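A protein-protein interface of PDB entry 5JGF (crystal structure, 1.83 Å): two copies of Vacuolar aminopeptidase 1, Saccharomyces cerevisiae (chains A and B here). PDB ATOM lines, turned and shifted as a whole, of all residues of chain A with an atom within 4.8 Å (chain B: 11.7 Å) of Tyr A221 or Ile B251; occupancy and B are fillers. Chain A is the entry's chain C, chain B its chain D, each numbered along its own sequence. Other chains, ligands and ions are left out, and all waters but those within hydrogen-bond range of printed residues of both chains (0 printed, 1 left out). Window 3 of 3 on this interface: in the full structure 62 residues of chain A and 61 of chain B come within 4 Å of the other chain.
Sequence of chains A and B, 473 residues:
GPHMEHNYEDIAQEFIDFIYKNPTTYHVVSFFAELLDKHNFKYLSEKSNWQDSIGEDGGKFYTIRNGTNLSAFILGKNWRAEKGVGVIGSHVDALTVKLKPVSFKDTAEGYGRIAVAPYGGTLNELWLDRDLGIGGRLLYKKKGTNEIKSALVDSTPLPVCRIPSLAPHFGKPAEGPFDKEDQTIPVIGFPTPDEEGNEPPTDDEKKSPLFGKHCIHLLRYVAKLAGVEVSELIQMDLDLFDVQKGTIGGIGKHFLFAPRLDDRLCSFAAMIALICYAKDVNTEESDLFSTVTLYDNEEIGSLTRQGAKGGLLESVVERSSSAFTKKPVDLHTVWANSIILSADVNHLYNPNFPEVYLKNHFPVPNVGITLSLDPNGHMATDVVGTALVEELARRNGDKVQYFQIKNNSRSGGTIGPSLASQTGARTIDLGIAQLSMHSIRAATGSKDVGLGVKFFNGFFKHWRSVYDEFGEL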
ATOM      1  N   ILE A 134      10.133 -16.778  30.064  1.00  0.00           N
ATOM      2  CA  ILE A 134      11.566 -16.734  30.319  1.00  0.00           C
ATOM      3  C   ILE A 134      12.103 -15.419  29.760  1.00  0.00           C
ATOM      4  O   ILE A 134      11.595 -14.908  28.763  1.00  0.00           O
ATOM      5  CB  ILE A 134      12.282 -17.947  29.664  1.00  0.00           C
ATOM      6  CG1 ILE A 134      13.759 -17.969  30.066  1.00  0.00           C
ATOM      7  CG2 ILE A 134      12.129 -17.898  28.144  1.00  0.00           C
ATOM      8  CD1 ILE A 134      14.475 -19.268  29.687  1.00  0.00           C
ATOM      9  N   SER A 155      10.078 -13.787  26.598  1.00  0.00           N
ATOM     10  CA  SER A 155       9.161 -14.639  25.843  1.00  0.00           C
ATOM     11  C   SER A 155       7.703 -14.204  25.910  1.00  0.00           C
ATOM     12  O   SER A 155       6.879 -14.665  25.119  1.00  0.00           O
ATOM     13  CB  SER A 155       9.263 -16.088  26.331  1.00  0.00           C
ATOM     14  OG  SER A 155       8.617 -16.241  27.584  1.00  0.00           O
ATOM     15  N   LEU A 158       4.387 -15.779  25.559  1.00  0.00           N
ATOM     16  CA  LEU A 158       4.560 -17.226  25.555  1.00  0.00           C
ATOM     17  C   LEU A 158       5.109 -17.795  26.857  1.00  0.00           C
ATOM     18  O   LEU A 158       6.227 -17.472  27.261  1.00  0.00           O
ATOM     19  CB  LEU A 158       5.489 -17.663  24.414  1.00  0.00           C
ATOM     20  CG  LEU A 158       5.800 -19.169  24.394  1.00  0.00           C
ATOM     21  CD1 LEU A 158       4.534 -19.948  24.045  1.00  0.00           C
ATOM     22  CD2 LEU A 158       6.901 -19.467  23.392  1.00  0.00           C
ATOM     23  N   VAL A 160       6.863 -20.453  28.363  1.00  0.00           N
ATOM     24  CA  VAL A 160       7.657 -21.600  27.934  1.00  0.00           C
ATOM     25  C   VAL A 160       7.753 -22.715  28.972  1.00  0.00           C
ATOM     26  O   VAL A 160       8.018 -23.862  28.622  1.00  0.00           O
ATOM     27  CB  VAL A 160       9.108 -21.178  27.556  1.00  0.00           C
ATOM     28  CG1 VAL A 160       9.083 -20.089  26.486  1.00  0.00           C
ATOM     29  CG2 VAL A 160       9.860 -20.686  28.794  1.00  0.00           C
ATOM     30  N   ILE A 188       9.472 -27.766  30.174  1.00  0.00           N
ATOM     31  CA  ILE A 188       9.504 -26.831  29.059  1.00  0.00           C
ATOM     32  C   ILE A 188       8.949 -27.369  27.738  1.00  0.00           C
ATOM     33  O   ILE A 188       8.638 -26.596  26.830  1.00  0.00           O
ATOM     34  CB  ILE A 188      10.950 -26.301  28.868  1.00  0.00           C
ATOM     35  CG1 ILE A 188      10.950 -25.091  27.935  1.00  0.00           C
ATOM     36  CG2 ILE A 188      11.851 -27.414  28.345  1.00  0.00           C
ATOM     37  CD1 ILE A 188      12.231 -24.278  28.006  1.00  0.00           C
ATOM     38  N   HIS A 217      17.544 -26.280  21.798  1.00  0.00           N
ATOM     39  CA  HIS A 217      16.248 -25.671  21.514  1.00  0.00           C
ATOM     40  C   HIS A 217      16.144 -24.335  22.249  1.00  0.00           C
ATOM     41  O   HIS A 217      15.684 -23.339  21.687  1.00  0.00           O
ATOM     42  CB  HIS A 217      15.122 -26.595  21.950  1.00  0.00           C
ATOM     43  N   LEU A 218      16.573 -24.309  23.506  1.00  0.00           N
ATOM     44  CA  LEU A 218      16.522 -23.071  24.277  1.00  0.00           C
ATOM     45  C   LEU A 218      17.483 -22.038  23.696  1.00  0.00           C
ATOM     46  O   LEU A 218      17.133 -20.864  23.557  1.00  0.00           O
ATOM     47  CB  LEU A 218      16.872 -23.337  25.743  1.00  0.00           C
ATOM     48  CG  LEU A 218      16.960 -22.096  26.640  1.00  0.00           C
ATOM     49  CD1 LEU A 218      15.634 -21.355  26.627  1.00  0.00           C
ATOM     50  CD2 LEU A 218      17.322 -22.514  28.056  1.00  0.00           C
ATOM     51  N   LEU A 219      18.694 -22.471  23.353  1.00  0.00           N
ATOM     52  CA  LEU A 219      19.682 -21.560  22.784  1.00  0.00           C
ATOM     53  C   LEU A 219      19.172 -20.934  21.488  1.00  0.00           C
ATOM     54  O   LEU A 219      19.305 -19.727  21.277  1.00  0.00           O
ATOM     55  CB  LEU A 219      21.004 -22.292  22.534  1.00  0.00           C
ATOM     56  CG  LEU A 219      21.811 -22.666  23.785  1.00  0.00           C
ATOM     57  CD1 LEU A 219      23.109 -23.352  23.380  1.00  0.00           C
ATOM     58  CD2 LEU A 219      22.106 -21.407  24.592  1.00  0.00           C
ATOM     59  N   ARG A 220      18.585 -21.754  20.624  1.00  0.00           N
ATOM     60  CA  ARG A 220      18.051 -21.258  19.362  1.00  0.00           C
ATOM     61  C   ARG A 220      16.944 -20.241  19.618  1.00  0.00           C
ATOM     62  O   ARG A 220      16.870 -19.208  18.955  1.00  0.00           O
ATOM     63  CB  ARG A 220      17.498 -22.413  18.527  1.00  0.00           C
ATOM     64  CG  ARG A 220      18.572 -23.270  17.882  1.00  0.00           C
ATOM     65  CD  ARG A 220      17.987 -24.554  17.317  1.00  0.00           C
ATOM     66  NE  ARG A 220      19.006 -25.361  16.657  1.00  0.00           N
ATOM     67  CZ  ARG A 220      18.843 -26.632  16.308  1.00  0.00           C
ATOM     68  NH1 ARG A 220      17.696 -27.248  16.558  1.00  0.00           N
ATOM     69  NH2 ARG A 220      19.827 -27.287  15.707  1.00  0.00           N
ATOM     70  N   TYR A 221      16.091 -20.534  20.595  1.00  0.00           N
ATOM     71  CA  TYR A 221      14.980 -19.649  20.924  1.00  0.00           C
ATOM     72  C   TYR A 221      15.409 -18.266  21.412  1.00  0.00           C
ATOM     73  O   TYR A 221      14.938 -17.251  20.893  1.00  0.00           O
ATOM     74  CB  TYR A 221      14.073 -20.313  21.965  1.00  0.00           C
ATOM     75  CG  TYR A 221      12.867 -19.480  22.342  1.00  0.00           C
ATOM     76  CD1 TYR A 221      12.793 -18.840  23.580  1.00  0.00           C
ATOM     77  CD2 TYR A 221      11.808 -19.309  21.449  1.00  0.00           C
ATOM     78  CE1 TYR A 221      11.691 -18.051  23.920  1.00  0.00           C
ATOM     79  CE2 TYR A 221      10.704 -18.521  21.777  1.00  0.00           C
ATOM     80  CZ  TYR A 221      10.653 -17.895  23.010  1.00  0.00           C
ATOM     81  OH  TYR A 221       9.570 -17.111  23.323  1.00  0.00           O
ATOM     82  N   VAL A 222      16.298 -18.210  22.401  1.00  0.00           N
ATOM     83  CA  VAL A 222      16.731 -16.912  22.905  1.00  0.00           C
ATOM     84  C   VAL A 222      17.575 -16.168  21.874  1.00  0.00           C
ATOM     85  O   VAL A 222      17.569 -14.937  21.830  1.00  0.00           O
ATOM     86  CB  VAL A 222      17.513 -17.038  24.243  1.00  0.00           C
ATOM     87  CG1 VAL A 222      16.614 -17.676  25.302  1.00  0.00           C
ATOM     88  CG2 VAL A 222      18.780 -17.848  24.051  1.00  0.00           C
ATOM     89  N   ALA A 223      18.290 -16.913  21.035  1.00  0.00           N
ATOM     90  CA  ALA A 223      19.104 -16.289  19.996  1.00  0.00           C
ATOM     91  C   ALA A 223      18.159 -15.589  19.023  1.00  0.00           C
ATOM     92  O   ALA A 223      18.413 -14.469  18.587  1.00  0.00           O
ATOM     93  CB  ALA A 223      19.924 -17.340  19.268  1.00  0.00           C
ATOM     94  N   LYS A 224      17.059 -16.259  18.698  1.00  0.00           N
ATOM     95  CA  LYS A 224      16.063 -15.708  17.787  1.00  0.00           C
ATOM     96  C   LYS A 224      15.427 -14.445  18.371  1.00  0.00           C
ATOM     97  O   LYS A 224      15.211 -13.465  17.660  1.00  0.00           O
ATOM     98  CB  LYS A 224      14.990 -16.753  17.497  1.00  0.00           C
ATOM     99  N   LEU A 225      15.132 -14.467  19.668  1.00  0.00           N
ATOM    100  CA  LEU A 225      14.528 -13.311  20.323  1.00  0.00           C
ATOM    101  C   LEU A 225      15.476 -12.117  20.323  1.00  0.00           C
ATOM    102  O   LEU A 225      15.042 -10.973  20.179  1.00  0.00           O
ATOM    103  CB  LEU A 225      14.150 -13.643  21.770  1.00  0.00           C
ATOM    104  CG  LEU A 225      13.053 -14.681  22.021  1.00  0.00           C
ATOM    105  CD1 LEU A 225      12.869 -14.858  23.517  1.00  0.00           C
ATOM    106  CD2 LEU A 225      11.748 -14.236  21.376  1.00  0.00           C
ATOM    107  N   THR B 247      -4.010 -20.975  27.660  1.00  0.00           N
ATOM    108  CA  THR B 247      -2.947 -20.588  26.747  1.00  0.00           C
ATOM    109  C   THR B 247      -2.172 -21.788  26.212  1.00  0.00           C
ATOM    110  O   THR B 247      -2.050 -22.816  26.881  1.00  0.00           O
ATOM    111  CB  THR B 247      -1.923 -19.675  27.457  1.00  0.00           C
ATOM    112  OG1 THR B 247      -2.607 -18.611  28.131  1.00  0.00           O
ATOM    113  CG2 THR B 247      -0.943 -19.087  26.449  1.00  0.00           C
ATOM    114  N   ILE B 248      -1.655 -21.655  24.996  1.00  0.00           N
ATOM    115  CA  ILE B 248      -0.831 -22.704  24.418  1.00  0.00           C
ATOM    116  C   ILE B 248       0.548 -22.399  24.994  1.00  0.00           C
ATOM    117  O   ILE B 248       1.000 -21.256  24.938  1.00  0.00           O
ATOM    118  CB  ILE B 248      -0.791 -22.611  22.875  1.00  0.00           C
ATOM    119  CG1 ILE B 248      -2.166 -22.961  22.306  1.00  0.00           C
ATOM    120  CG2 ILE B 248       0.278 -23.543  22.315  1.00  0.00           C
ATOM    121  CD1 ILE B 248      -2.679 -24.336  22.732  1.00  0.00           C
ATOM    122  N   GLY B 249       1.210 -23.405  25.556  1.00  0.00           N
ATOM    123  CA  GLY B 249       2.509 -23.168  26.158  1.00  0.00           C
ATOM    124  C   GLY B 249       3.597 -24.166  25.833  1.00  0.00           C
ATOM    125  O   GLY B 249       3.392 -25.121  25.079  1.00  0.00           O
ATOM    126  N   GLY B 250       4.763 -23.944  26.434  1.00  0.00           N
ATOM    127  CA  GLY B 250       5.906 -24.796  26.188  1.00  0.00           C
ATOM    128  C   GLY B 250       6.746 -24.079  25.152  1.00  0.00           C
ATOM    129  O   GLY B 250       6.203 -23.377  24.298  1.00  0.00           O
ATOM    130  N   ILE B 251       8.061 -24.238  25.218  1.00  0.00           N
ATOM    131  CA  ILE B 251       8.939 -23.567  24.269  1.00  0.00           C
ATOM    132  C   ILE B 251       8.627 -23.959  22.822  1.00  0.00           C
ATOM    133  O   ILE B 251       8.876 -23.185  21.893  1.00  0.00           O
ATOM    134  CB  ILE B 251      10.428 -23.856  24.592  1.00  0.00           C
ATOM    135  CG1 ILE B 251      11.314 -22.815  23.908  1.00  0.00           C
ATOM    136  CG2 ILE B 251      10.804 -25.264  24.154  1.00  0.00           C
ATOM    137  CD1 ILE B 251      12.745 -22.799  24.418  1.00  0.00           C
ATOM    138  N   GLY B 252       8.070 -25.155  22.643  1.00  0.00           N
ATOM    139  CA  GLY B 252       7.716 -25.629  21.316  1.00  0.00           C
ATOM    140  C   GLY B 252       6.210 -25.714  21.127  1.00  0.00           C
ATOM    141  O   GLY B 252       5.726 -26.366  20.199  1.00  0.00           O
ATOM    142  N   LYS B 253       5.473 -25.048  22.014  1.00  0.00           N
ATOM    143  CA  LYS B 253       4.013 -25.020  21.983  1.00  0.00           C
ATOM    144  C   LYS B 253       3.378 -26.409  22.011  1.00  0.00           C
ATOM    145  O   LYS B 253       2.370 -26.661  21.348  1.00  0.00           O
ATOM    146  CB  LYS B 253       3.530 -24.229  20.759  1.00  0.00           C
ATOM    147  CG  LYS B 253       3.976 -22.774  20.785  1.00  0.00           C
ATOM    148  CD  LYS B 253       3.318 -21.941  19.699  1.00  0.00           C
ATOM    149  CE  LYS B 253       3.698 -20.475  19.850  1.00  0.00           C
ATOM    150  NZ  LYS B 253       3.038 -19.597  18.843  1.00  0.00           N
ATOM    151  N   HIS B 254       3.967 -27.293  22.811  1.00  0.00           N
ATOM    152  CA  HIS B 254       3.503 -28.671  22.962  1.00  0.00           C
ATOM    153  C   HIS B 254       2.375 -28.810  23.978  1.00  0.00           C
ATOM    154  O   HIS B 254       1.728 -29.856  24.044  1.00  0.00           O
ATOM    155  CB  HIS B 254       4.650 -29.565  23.437  1.00  0.00           C
ATOM    156  CG  HIS B 254       5.783 -29.670  22.467  1.00  0.00           C
ATOM    157  ND1 HIS B 254       7.101 -29.553  22.853  1.00  0.00           N
ATOM    158  CD2 HIS B 254       5.798 -29.906  21.135  1.00  0.00           C
ATOM    159  CE1 HIS B 254       7.881 -29.714  21.798  1.00  0.00           C
ATOM    160  NE2 HIS B 254       7.115 -29.929  20.742  1.00  0.00           N
ATOM    161  N   PHE B 255       2.147 -27.765  24.766  1.00  0.00           N
ATOM    162  CA  PHE B 255       1.136 -27.812  25.818  1.00  0.00           C
ATOM    163  C   PHE B 255      -0.011 -26.821  25.719  1.00  0.00           C
ATOM    164  O   PHE B 255       0.059 -25.819  25.009  1.00  0.00           O
ATOM    165  CB  PHE B 255       1.805 -27.597  27.180  1.00  0.00           C
ATOM    166  CG  PHE B 255       2.874 -28.599  27.497  1.00  0.00           C
ATOM    167  CD1 PHE B 255       2.547 -29.922  27.767  1.00  0.00           C
ATOM    168  CD2 PHE B 255       4.213 -28.217  27.526  1.00  0.00           C
ATOM    169  CE1 PHE B 255       3.539 -30.854  28.061  1.00  0.00           C
ATOM    170  CE2 PHE B 255       5.214 -29.143  27.821  1.00  0.00           C
ATOM    171  CZ  PHE B 255       4.875 -30.461  28.088  1.00  0.00           C
ATOM    172  N   LEU B 256      -1.061 -27.123  26.477  1.00  0.00           N
ATOM    173  CA  LEU B 256      -2.244 -26.282  26.577  1.00  0.00           C
ATOM    174  C   LEU B 256      -2.497 -26.169  28.078  1.00  0.00           C
ATOM    175  O   LEU B 256      -2.683 -27.181  28.756  1.00  0.00           O
ATOM    176  CB  LEU B 256      -3.444 -26.936  25.877  1.00  0.00           C
ATOM    177  CG  LEU B 256      -4.763 -26.143  25.818  1.00  0.00           C
ATOM    178  CD1 LEU B 256      -5.643 -26.694  24.707  1.00  0.00           C
ATOM    179  CD2 LEU B 256      -5.493 -26.225  27.150  1.00  0.00           C
ATOM    180  N   PHE B 257      -2.459 -24.943  28.595  1.00  0.00           N
ATOM    181  CA  PHE B 257      -2.687 -24.694  30.014  1.00  0.00           C
ATOM    182  C   PHE B 257      -4.069 -24.073  30.142  1.00  0.00           C
ATOM    183  O   PHE B 257      -4.383 -23.105  29.452  1.00  0.00           O
ATOM    184  CB  PHE B 257      -1.651 -23.710  30.580  1.00  0.00           C
ATOM    185  CG  PHE B 257      -0.217 -24.081  30.291  1.00  0.00           C
ATOM    186  CD1 PHE B 257       0.188 -25.410  30.261  1.00  0.00           C
ATOM    187  CD2 PHE B 257       0.740 -23.087  30.104  1.00  0.00           C
ATOM    188  CE1 PHE B 257       1.527 -25.746  30.052  1.00  0.00           C
ATOM    189  CE2 PHE B 257       2.083 -23.412  29.895  1.00  0.00           C
ATOM    190  CZ  PHE B 257       2.476 -24.743  29.870  1.00  0.00           C
ATOM    191  N   ASN B 366       0.260 -35.505  23.510  1.00  0.00           N
ATOM    192  CA  ASN B 366       0.111 -35.519  22.057  1.00  0.00           C
ATOM    193  C   ASN B 366       0.255 -36.837  21.307  1.00  0.00           C
ATOM    194  O   ASN B 366       0.749 -36.864  20.176  1.00  0.00           O
ATOM    195  CB  ASN B 366       1.072 -34.480  21.473  1.00  0.00           C
ATOM    196  CG  ASN B 366       0.923 -33.128  22.144  1.00  0.00           C
ATOM    197  OD1 ASN B 366      -0.185 -32.612  22.274  1.00  0.00           O
ATOM    198  ND2 ASN B 366       2.036 -32.550  22.578  1.00  0.00           N
ATOM    199  N   THR B 444      -2.438 -30.117  29.437  1.00  0.00           N
ATOM    200  CA  THR B 444      -2.504 -31.309  28.607  1.00  0.00           C
ATOM    201  C   THR B 444      -1.726 -30.979  27.334  1.00  0.00           C
ATOM    202  O   THR B 444      -1.150 -29.895  27.229  1.00  0.00           O
ATOM    203  CB  THR B 444      -3.975 -31.695  28.278  1.00  0.00           C
ATOM    204  OG1 THR B 444      -3.997 -32.943  27.573  1.00  0.00           O
ATOM    205  CG2 THR B 444      -4.649 -30.618  27.438  1.00  0.00           C
ATOM    206  N   GLY B 445      -1.675 -31.909  26.386  1.00  0.00           N
ATOM    207  CA  GLY B 445      -0.955 -31.636  25.157  1.00  0.00           C
ATOM    208  C   GLY B 445      -1.772 -30.715  24.269  1.00  0.00           C
ATOM    209  O   GLY B 445      -2.998 -30.789  24.260  1.00  0.00           O
ATOM    210  N   SER B 446      -1.102 -29.844  23.518  1.00  0.00           N
ATOM    211  CA  SER B 446      -1.816 -28.932  22.623  1.00  0.00           C
ATOM    212  C   SER B 446      -2.522 -29.681  21.481  1.00  0.00           C
ATOM    213  O   SER B 446      -3.463 -29.157  20.885  1.00  0.00           O
ATOM    214  CB  SER B 446      -0.854 -27.889  22.054  1.00  0.00           C
ATOM    215  OG  SER B 446       0.237 -28.503  21.390  1.00  0.00           O
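The backbone carbonyl oxygen (O) of Val A160 is in hydrogen-bond range of the backbone NH (N) of Ile B251 (3.4 Å).
O of Ile A188 is in hydrogen-bond range of N of Ile B251.
OG of Ser A155 lies within hydrogen-bond range of O of Leu A158 (2.7 Å).
Among the printed residues, merely in contact across the chains: Leu A158 with Ile B248, Leu A158 with Gly B250, Val A160 with Gly B250, Ile A188 with Gly B250, Leu A218 with Ile B251 and Tyr A221 with Ile B251.
No residue of chain B comes within 4 Å of Ile A134.
No residue of chain B comes within 4 Å of Ser A155.
Leu A158 touches just these residues of chain B: Ile B248 (3.9 Å) and Gly B250 (3.8 Å).
Of chain B, only Gly B250 (3.4 Å) and Ile B251 (3.4 Å) come within 4 Å of Val A160.
Of chain B, only Gly B250 (3.3 Å) and Ile B251 (2.9 Å) come within 4 Å of Ile A188.
Leu A218 touches just one residue of chain B: Ile B251.
Tyr A221 touches one residue of chain B.
Ala A223 touches none of the printed residues of chain B.
No residue of chain B comes within 4 Å of Lys A224.
No residue of chain B comes within 4 Å of Leu A225.
Thr B247 touches none of the printed residues of chain A.
Of the printed residues of chain A, Ile B248 touches Leu A158 (3.9 Å).
Printed residues of chain A within 4 Å of Gly B250: Leu A158 (3.8 Å), Val A160 (3.4 Å) and Ile A188 (3.3 Å).
Of the printed residues of chain A, Ile B251 touches Val A160 (3.4 Å), Ile A188 (2.9 Å), Leu A218 (3.8 Å) and Tyr A221 (3.7 Å).
The nearest residue of chain B that does not touch Tyr A221 is Gly B252 (7.0 Å).
Hydrophobic or aromatic side chains of chain A that line the printed part of chain B: Leu A158, Val A160, Ile A188, Leu A218 and Tyr A221.
Of the 15 printed residues of chain B, 3 touch a printed residue of chain A.
Along chain B the printed residues that touch a printed residue of chain A span positions 248 to 251.
Among the printed residues, no Asp or Glu carboxylate lies within 4 Å of a Lys or Arg side-chain nitrogen of the other chain.
No position is printed for both chains.
Of the 8 pairs that touch across the chains among the printed residues, none has its exchanged pair printed and touching as well.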
